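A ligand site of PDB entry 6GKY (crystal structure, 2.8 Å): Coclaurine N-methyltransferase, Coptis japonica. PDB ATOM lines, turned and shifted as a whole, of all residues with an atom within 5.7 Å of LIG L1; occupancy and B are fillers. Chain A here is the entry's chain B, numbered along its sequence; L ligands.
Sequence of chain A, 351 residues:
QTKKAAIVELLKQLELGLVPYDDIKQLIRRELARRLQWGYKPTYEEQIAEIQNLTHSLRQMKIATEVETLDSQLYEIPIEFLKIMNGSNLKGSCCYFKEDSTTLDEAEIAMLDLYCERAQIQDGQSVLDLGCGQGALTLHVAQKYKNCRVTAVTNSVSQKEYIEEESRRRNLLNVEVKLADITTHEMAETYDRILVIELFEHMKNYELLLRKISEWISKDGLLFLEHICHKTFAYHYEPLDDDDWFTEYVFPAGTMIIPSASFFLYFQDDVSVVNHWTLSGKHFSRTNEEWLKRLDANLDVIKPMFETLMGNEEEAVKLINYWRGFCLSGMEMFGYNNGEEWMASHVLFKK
The backbone carbonyl oxygen (O) of Phe 284 is in hydrogen-bond range of the side-chain amide nitrogen (ND2) of Asn 288.
The backbone NH (N) of Ile 228 lies within hydrogen-bond range of the side-chain carboxylate (OE2) of Glu 201 (3.1 Å).
O of Met 256 lies within hydrogen-bond range of N of Tyr 237 (3.2 Å).
The side-chain sulfur (SD) of Met 333 lies close to the side-chain hydroxyl (OH) of Tyr 237 (3.3 Å).
Residues that only touch LIG L1: Gly 92 (3.9 Å), Ile 228 (3.6 Å), Phe 251 (3.4 Å), Met 256 (3.8 Å), Phe 284 (3.5 Å), Phe 326 (3.9 Å), Gly 330 (3.96 Å), Met 333 (3.9 Å) and Phe 334 (3.7 Å).
Hydrophobic or aromatic side chains that line LIG L1: His 202, Ile 228, Phe 251, Met 256, Phe 284, Phe 326, Met 333 and Phe 334.
Within 4 Å of LIG L1: Tyr 75, Gly 92, Glu 198, His 202, Ile 228, Phe 251, Met 256, Phe 284, Phe 326, Gly 330, Met 333 and Phe 334.
Along chain A the residues within 4 Å of LIG L1 span positions 75 to 334.
The nearest printed residue that does not touch LIG L1 is Ile 258 (4.02 Å).
A ring nitrogen (NE2) of His 202 is in hydrogen-bond range of an oxygen (O2) of LIG L1 (3.3 Å).
OH of Tyr 75 lies within hydrogen-bond range of O2 of LIG L1 (3.4 Å).
N1 of LIG L1 is in hydrogen-bond range of OE1 of Glu 198 (3.4 Å).
A sulfur (S1) of LG2 L2 sits close to the side-chain hydroxyl (OH) of Tyr 75.
N of Gly 92 is in hydrogen-bond range of O2 of LG2 L2 (3.1 Å).
The side-chain hydroxyl (OG) of Ser 93 sits at hydrogen-bond distance from an oxygen (O1) of LG2 L2, 2.7 Å away.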
ATOM      1  N   TYR A  75     -27.897  25.002  14.453  1.00  0.00           N
ATOM      2  CA  TYR A  75     -28.750  23.805  14.583  1.00  0.00           C
ATOM      3  C   TYR A  75     -29.331  23.094  13.339  1.00  0.00           C
ATOM      4  O   TYR A  75     -29.828  21.973  13.462  1.00  0.00           O
ATOM      5  CB  TYR A  75     -29.911  24.154  15.514  1.00  0.00           C
ATOM      6  CG  TYR A  75     -29.493  24.696  16.855  1.00  0.00           C
ATOM      7  CD1 TYR A  75     -28.484  24.082  17.572  1.00  0.00           C
ATOM      8  CD2 TYR A  75     -30.096  25.828  17.396  1.00  0.00           C
ATOM      9  CE1 TYR A  75     -28.091  24.577  18.797  1.00  0.00           C
ATOM     10  CE2 TYR A  75     -29.703  26.324  18.622  1.00  0.00           C
ATOM     11  CZ  TYR A  75     -28.697  25.688  19.325  1.00  0.00           C
ATOM     12  OH  TYR A  75     -28.285  26.159  20.547  1.00  0.00           O
ATOM     13  N   GLY A  92     -24.772  17.730  21.638  1.00  0.00           N
ATOM     14  CA  GLY A  92     -24.361  19.090  21.346  1.00  0.00           C
ATOM     15  C   GLY A  92     -24.334  19.978  22.576  1.00  0.00           C
ATOM     16  O   GLY A  92     -24.456  21.193  22.471  1.00  0.00           O
ATOM     17  N   SER A  93     -24.165  19.359  23.742  1.00  0.00           N
ATOM     18  CA  SER A  93     -24.123  20.088  25.002  1.00  0.00           C
ATOM     19  C   SER A  93     -22.988  19.593  25.879  1.00  0.00           C
ATOM     20  O   SER A  93     -22.186  18.762  25.467  1.00  0.00           O
ATOM     21  CB  SER A  93     -25.461  19.961  25.730  1.00  0.00           C
ATOM     22  OG  SER A  93     -25.810  18.603  25.939  1.00  0.00           O
ATOM     23  N   GLU A 198     -30.080  22.946  28.061  1.00  0.00           N
ATOM     24  CA  GLU A 198     -29.487  24.102  27.403  1.00  0.00           C
ATOM     25  C   GLU A 198     -30.390  24.659  26.301  1.00  0.00           C
ATOM     26  O   GLU A 198     -29.977  24.789  25.150  1.00  0.00           O
ATOM     27  CB  GLU A 198     -28.110  23.739  26.823  1.00  0.00           C
ATOM     28  CG  GLU A 198     -27.115  23.278  27.862  1.00  0.00           C
ATOM     29  CD  GLU A 198     -25.728  23.034  27.297  1.00  0.00           C
ATOM     30  OE1 GLU A 198     -25.522  23.322  26.093  1.00  0.00           O
ATOM     31  OE2 GLU A 198     -24.849  22.573  28.038  1.00  0.00           O
ATOM     32  N   LEU A 199     -31.619  24.997  26.680  1.00  0.00           N
ATOM     33  CA  LEU A 199     -32.584  25.551  25.742  1.00  0.00           C
ATOM     34  C   LEU A 199     -32.983  26.971  26.139  1.00  0.00           C
ATOM     35  O   LEU A 199     -33.310  27.788  25.287  1.00  0.00           O
ATOM     36  CB  LEU A 199     -33.835  24.658  25.665  1.00  0.00           C
ATOM     37  CG  LEU A 199     -35.022  25.207  24.877  1.00  0.00           C
ATOM     38  CD1 LEU A 199     -34.715  25.249  23.386  1.00  0.00           C
ATOM     39  CD2 LEU A 199     -36.279  24.390  25.153  1.00  0.00           C
ATOM     40  N   GLU A 201     -31.211  29.324  27.254  1.00  0.00           N
ATOM     41  CA  GLU A 201     -30.237  30.335  26.854  1.00  0.00           C
ATOM     42  C   GLU A 201     -30.717  31.077  25.606  1.00  0.00           C
ATOM     43  O   GLU A 201     -30.332  32.218  25.359  1.00  0.00           O
ATOM     44  CB  GLU A 201     -28.867  29.699  26.594  1.00  0.00           C
ATOM     45  CG  GLU A 201     -28.221  29.054  27.806  1.00  0.00           C
ATOM     46  CD  GLU A 201     -28.772  27.668  28.080  1.00  0.00           C
ATOM     47  OE1 GLU A 201     -29.901  27.383  27.650  1.00  0.00           O
ATOM     48  OE2 GLU A 201     -28.055  26.862  28.715  1.00  0.00           O
ATOM     49  N   HIS A 202     -31.568  30.407  24.823  1.00  0.00           N
ATOM     50  CA  HIS A 202     -32.080  30.976  23.575  1.00  0.00           C
ATOM     51  C   HIS A 202     -33.392  31.717  23.775  1.00  0.00           C
ATOM     52  O   HIS A 202     -33.869  32.420  22.885  1.00  0.00           O
ATOM     53  CB  HIS A 202     -32.270  29.863  22.536  1.00  0.00           C
ATOM     54  CG  HIS A 202     -30.999  29.176  22.152  1.00  0.00           C
ATOM     55  ND1 HIS A 202     -29.905  29.857  21.665  1.00  0.00           N
ATOM     56  CD2 HIS A 202     -30.651  27.863  22.164  1.00  0.00           C
ATOM     57  CE1 HIS A 202     -28.931  28.991  21.403  1.00  0.00           C
ATOM     58  NE2 HIS A 202     -29.365  27.782  21.705  1.00  0.00           N
ATOM     59  N   ILE A 228     -25.889  26.451  30.960  1.00  0.00           N
ATOM     60  CA  ILE A 228     -24.583  27.015  31.235  1.00  0.00           C
ATOM     61  C   ILE A 228     -24.776  28.393  31.850  1.00  0.00           C
ATOM     62  O   ILE A 228     -25.814  29.029  31.672  1.00  0.00           O
ATOM     63  CB  ILE A 228     -23.709  27.102  29.978  1.00  0.00           C
ATOM     64  CG1 ILE A 228     -24.418  27.891  28.877  1.00  0.00           C
ATOM     65  CG2 ILE A 228     -23.353  25.714  29.476  1.00  0.00           C
ATOM     66  CD1 ILE A 228     -23.959  29.324  28.794  1.00  0.00           C
ATOM     67  N   TYR A 237     -26.137  38.452  25.734  1.00  0.00           N
ATOM     68  CA  TYR A 237     -24.869  38.391  25.016  1.00  0.00           C
ATOM     69  C   TYR A 237     -24.820  39.434  23.913  1.00  0.00           C
ATOM     70  O   TYR A 237     -24.915  39.116  22.728  1.00  0.00           O
ATOM     71  CB  TYR A 237     -24.607  36.997  24.467  1.00  0.00           C
ATOM     72  CG  TYR A 237     -23.466  36.311  25.188  1.00  0.00           C
ATOM     73  CD1 TYR A 237     -23.351  36.427  26.570  1.00  0.00           C
ATOM     74  CD2 TYR A 237     -22.519  35.582  24.501  1.00  0.00           C
ATOM     75  CE1 TYR A 237     -22.306  35.830  27.247  1.00  0.00           C
ATOM     76  CE2 TYR A 237     -21.468  34.967  25.175  1.00  0.00           C
ATOM     77  CZ  TYR A 237     -21.375  35.086  26.548  1.00  0.00           C
ATOM     78  OH  TYR A 237     -20.343  34.495  27.236  1.00  0.00           O
ATOM     79  N   VAL A 250     -19.243  33.943  17.768  1.00  0.00           N
ATOM     80  CA  VAL A 250     -19.813  32.641  17.468  1.00  0.00           C
ATOM     81  C   VAL A 250     -21.323  32.700  17.279  1.00  0.00           C
ATOM     82  O   VAL A 250     -21.837  32.306  16.233  1.00  0.00           O
ATOM     83  CB  VAL A 250     -19.498  31.621  18.588  1.00  0.00           C
ATOM     84  CG1 VAL A 250     -20.265  30.334  18.359  1.00  0.00           C
ATOM     85  CG2 VAL A 250     -17.996  31.353  18.650  1.00  0.00           C
ATOM     86  N   PHE A 251     -22.028  33.202  18.291  1.00  0.00           N
ATOM     87  CA  PHE A 251     -23.478  33.272  18.252  1.00  0.00           C
ATOM     88  C   PHE A 251     -23.964  34.584  17.660  1.00  0.00           C
ATOM     89  O   PHE A 251     -23.468  35.650  18.004  1.00  0.00           O
ATOM     90  CB  PHE A 251     -24.073  33.085  19.646  1.00  0.00           C
ATOM     91  CG  PHE A 251     -23.706  31.776  20.283  1.00  0.00           C
ATOM     92  CD1 PHE A 251     -22.609  31.680  21.121  1.00  0.00           C
ATOM     93  CD2 PHE A 251     -24.464  30.642  20.053  1.00  0.00           C
ATOM     94  CE1 PHE A 251     -22.272  30.485  21.714  1.00  0.00           C
ATOM     95  CE2 PHE A 251     -24.134  29.435  20.634  1.00  0.00           C
ATOM     96  CZ  PHE A 251     -23.031  29.352  21.474  1.00  0.00           C
ATOM     97  N   MET A 256     -28.567  34.816  22.359  1.00  0.00           N
ATOM     98  CA  MET A 256     -28.032  34.186  23.558  1.00  0.00           C
ATOM     99  C   MET A 256     -28.246  35.003  24.830  1.00  0.00           C
ATOM    100  O   MET A 256     -28.193  36.237  24.810  1.00  0.00           O
ATOM    101  CB  MET A 256     -26.543  33.894  23.376  1.00  0.00           C
ATOM    102  CG  MET A 256     -26.242  32.658  22.562  1.00  0.00           C
ATOM    103  SD  MET A 256     -26.589  31.146  23.488  1.00  0.00           S
ATOM    104  CE  MET A 256     -25.454  31.323  24.852  1.00  0.00           C
ATOM    105  N   ILE A 258     -26.831  34.632  28.968  1.00  0.00           N
ATOM    106  CA  ILE A 258     -26.073  33.886  29.972  1.00  0.00           C
ATOM    107  C   ILE A 258     -26.574  34.203  31.375  1.00  0.00           C
ATOM    108  O   ILE A 258     -26.256  35.260  31.927  1.00  0.00           O
ATOM    109  CB  ILE A 258     -24.575  34.184  29.883  1.00  0.00           C
ATOM    110  CG1 ILE A 258     -24.038  33.677  28.545  1.00  0.00           C
ATOM    111  CG2 ILE A 258     -23.836  33.547  31.052  1.00  0.00           C
ATOM    112  CD1 ILE A 258     -24.539  32.303  28.173  1.00  0.00           C
ATOM    113  N   PHE A 284     -17.311  21.427  30.380  1.00  0.00           N
ATOM    114  CA  PHE A 284     -17.676  21.942  29.058  1.00  0.00           C
ATOM    115  C   PHE A 284     -16.420  22.353  28.309  1.00  0.00           C
ATOM    116  O   PHE A 284     -16.338  22.224  27.078  1.00  0.00           O
ATOM    117  CB  PHE A 284     -18.664  23.112  29.177  1.00  0.00           C
ATOM    118  CG  PHE A 284     -19.562  23.276  27.986  1.00  0.00           C
ATOM    119  CD1 PHE A 284     -19.527  22.363  26.942  1.00  0.00           C
ATOM    120  CD2 PHE A 284     -20.438  24.343  27.906  1.00  0.00           C
ATOM    121  CE1 PHE A 284     -20.357  22.516  25.848  1.00  0.00           C
ATOM    122  CE2 PHE A 284     -21.259  24.500  26.811  1.00  0.00           C
ATOM    123  CZ  PHE A 284     -21.223  23.585  25.777  1.00  0.00           C
ATOM    124  N   ASN A 288     -15.489  20.949  24.531  1.00  0.00           N
ATOM    125  CA  ASN A 288     -15.138  21.718  23.331  1.00  0.00           C
ATOM    126  C   ASN A 288     -13.742  21.361  22.832  1.00  0.00           C
ATOM    127  O   ASN A 288     -13.471  21.413  21.637  1.00  0.00           O
ATOM    128  CB  ASN A 288     -15.223  23.214  23.613  1.00  0.00           C
ATOM    129  CG  ASN A 288     -16.651  23.718  23.668  1.00  0.00           C
ATOM    130  OD1 ASN A 288     -17.234  24.070  22.638  1.00  0.00           O
ATOM    131  ND2 ASN A 288     -17.222  23.760  24.868  1.00  0.00           N
ATOM    132  N   PHE A 326     -15.903  28.227  17.512  1.00  0.00           N
ATOM    133  CA  PHE A 326     -16.948  27.672  18.375  1.00  0.00           C
ATOM    134  C   PHE A 326     -16.323  26.881  19.510  1.00  0.00           C
ATOM    135  O   PHE A 326     -16.631  27.108  20.682  1.00  0.00           O
ATOM    136  CB  PHE A 326     -17.905  26.796  17.561  1.00  0.00           C
ATOM    137  CG  PHE A 326     -19.095  26.317  18.350  1.00  0.00           C
ATOM    138  CD1 PHE A 326     -20.254  27.079  18.415  1.00  0.00           C
ATOM    139  CD2 PHE A 326     -19.055  25.091  19.002  1.00  0.00           C
ATOM    140  CE1 PHE A 326     -21.349  26.633  19.133  1.00  0.00           C
ATOM    141  CE2 PHE A 326     -20.160  24.644  19.710  1.00  0.00           C
ATOM    142  CZ  PHE A 326     -21.301  25.412  19.775  1.00  0.00           C
ATOM    143  N   SER A 329     -14.022  29.179  21.695  1.00  0.00           N
ATOM    144  CA  SER A 329     -14.807  30.049  22.554  1.00  0.00           C
ATOM    145  C   SER A 329     -15.262  29.302  23.792  1.00  0.00           C
ATOM    146  O   SER A 329     -15.246  29.839  24.897  1.00  0.00           O
ATOM    147  CB  SER A 329     -16.009  30.610  21.799  1.00  0.00           C
ATOM    148  OG  SER A 329     -15.611  31.511  20.775  1.00  0.00           O
ATOM    149  N   GLY A 330     -15.679  28.049  23.613  1.00  0.00           N
ATOM    150  CA  GLY A 330     -16.137  27.224  24.710  1.00  0.00           C
ATOM    151  C   GLY A 330     -14.999  26.780  25.613  1.00  0.00           C
ATOM    152  O   GLY A 330     -15.166  26.676  26.828  1.00  0.00           O
ATOM    153  N   MET A 333     -13.529  30.078  27.616  1.00  0.00           N
ATOM    154  CA  MET A 333     -14.570  30.714  28.417  1.00  0.00           C
ATOM    155  C   MET A 333     -14.886  29.908  29.672  1.00  0.00           C
ATOM    156  O   MET A 333     -14.786  30.419  30.791  1.00  0.00           O
ATOM    157  CB  MET A 333     -15.843  30.915  27.600  1.00  0.00           C
ATOM    158  CG  MET A 333     -17.082  31.159  28.461  1.00  0.00           C
ATOM    159  SD  MET A 333     -18.457  31.815  27.504  1.00  0.00           S
ATOM    160  CE  MET A 333     -17.703  33.347  26.947  1.00  0.00           C
ATOM    161  N   PHE A 334     -15.259  28.650  29.490  1.00  0.00           N
ATOM    162  CA  PHE A 334     -15.668  27.806  30.613  1.00  0.00           C
ATOM    163  C   PHE A 334     -14.472  27.262  31.390  1.00  0.00           C
ATOM    164  O   PHE A 334     -14.623  26.851  32.546  1.00  0.00           O
ATOM    165  CB  PHE A 334     -16.535  26.650  30.112  1.00  0.00           C
ATOM    166  CG  PHE A 334     -17.864  27.092  29.570  1.00  0.00           C
ATOM    167  CD1 PHE A 334     -18.015  27.399  28.223  1.00  0.00           C
ATOM    168  CD2 PHE A 334     -18.967  27.197  30.398  1.00  0.00           C
ATOM    169  CE1 PHE A 334     -19.244  27.796  27.721  1.00  0.00           C
ATOM    170  CE2 PHE A 334     -20.189  27.606  29.907  1.00  0.00           C
ATOM    171  CZ  PHE A 334     -20.328  27.906  28.569  1.00  0.00           C
HETATM  172  C1  LIG L   1     -21.776  30.299  26.057  1.00  0.00           C
HETATM  173  O1  LIG L   1     -21.211  29.480  25.022  1.00  0.00           O
HETATM  174  C2  LIG L   1     -21.953  28.389  24.685  1.00  0.00           C
HETATM  175  C3  LIG L   1     -23.305  28.242  24.988  1.00  0.00           C
HETATM  176  C4  LIG L   1     -23.980  27.086  24.601  1.00  0.00           C
HETATM  177  C5  LIG L   1     -25.331  26.968  24.927  1.00  0.00           C
HETATM  178  C6  LIG L   1     -26.029  26.226  23.977  1.00  0.00           C
HETATM  179  O2  LIG L   1     -27.219  26.458  23.765  1.00  0.00           O
HETATM  180  N1  LIG L   1     -25.382  25.210  23.257  1.00  0.00           N
HETATM  181  C7  LIG L   1     -23.958  24.919  23.511  1.00  0.00           C
HETATM  182  C8  LIG L   1     -23.305  26.078  23.900  1.00  0.00           C
HETATM  183  C9  LIG L   1     -21.957  26.234  23.599  1.00  0.00           C
HETATM  184  C10 LIG L   1     -21.291  27.388  23.976  1.00  0.00           C
HETATM  185  O3  LIG L   1     -19.958  27.586  23.721  1.00  0.00           O
HETATM  186  C11 LIG L   1     -19.711  28.464  22.620  1.00  0.00           C
HETATM  187  N1  LG2 L   2     -30.634  19.214  23.956  1.00  0.00           N
HETATM  188  C1  LG2 L   2     -29.753  18.874  22.846  1.00  0.00           C
HETATM  189  C2  LG2 L   2     -29.452  20.101  21.998  1.00  0.00           C
HETATM  190  C3  LG2 L   2     -29.203  21.376  22.802  1.00  0.00           C
HETATM  191  S1  LG2 L   2     -28.831  22.788  21.742  1.00  0.00           S
HETATM  192  C4  LG2 L   2     -28.452  18.246  23.346  1.00  0.00           C
HETATM  193  O1  LG2 L   2     -28.116  18.341  24.523  1.00  0.00           O
HETATM  194  O2  LG2 L   2     -27.714  17.624  22.580  1.00  0.00           O
HETATM  195  C5  LG2 L   2     -30.500  23.430  22.026  1.00  0.00           C
HETATM  196  C6  LG2 L   2     -31.544  22.735  21.148  1.00  0.00           C
HETATM  197  O3  LG2 L   2     -32.798  23.375  21.293  1.00  0.00           O
HETATM  198  C7  LG2 L   2     -31.167  22.788  19.685  1.00  0.00           C
HETATM  199  O4  LG2 L   2     -30.940  21.490  19.200  1.00  0.00           O
HETATM  200  C8  LG2 L   2     -32.347  23.406  18.967  1.00  0.00           C
HETATM  201  O5  LG2 L   2     -32.777  22.572  17.913  1.00  0.00           O
HETATM  202  C9  LG2 L   2     -33.429  23.508  20.025  1.00  0.00           C
HETATM  203  N2  LG2 L   2     -34.141  24.798  19.925  1.00  0.00           N
HETATM  204  C10 LG2 L   2     -33.574  26.049  19.967  1.00  0.00           C
HETATM  205  N3  LG2 L   2     -34.555  26.966  19.842  1.00  0.00           N
HETATM  206  C11 LG2 L   2     -35.738  26.328  19.723  1.00  0.00           C
HETATM  207  C12 LG2 L   2     -37.034  26.793  19.565  1.00  0.00           C
HETATM  208  N4  LG2 L   2     -37.283  28.095  19.507  1.00  0.00           N
HETATM  209  N5  LG2 L   2     -38.075  25.881  19.466  1.00  0.00           N
HETATM  210  C13 LG2 L   2     -37.810  24.532  19.517  1.00  0.00           C
HETATM  211  N6  LG2 L   2     -36.518  24.079  19.667  1.00  0.00           N
HETATM  212  C14 LG2 L   2     -35.488  24.963  19.773  1.00  0.00           C
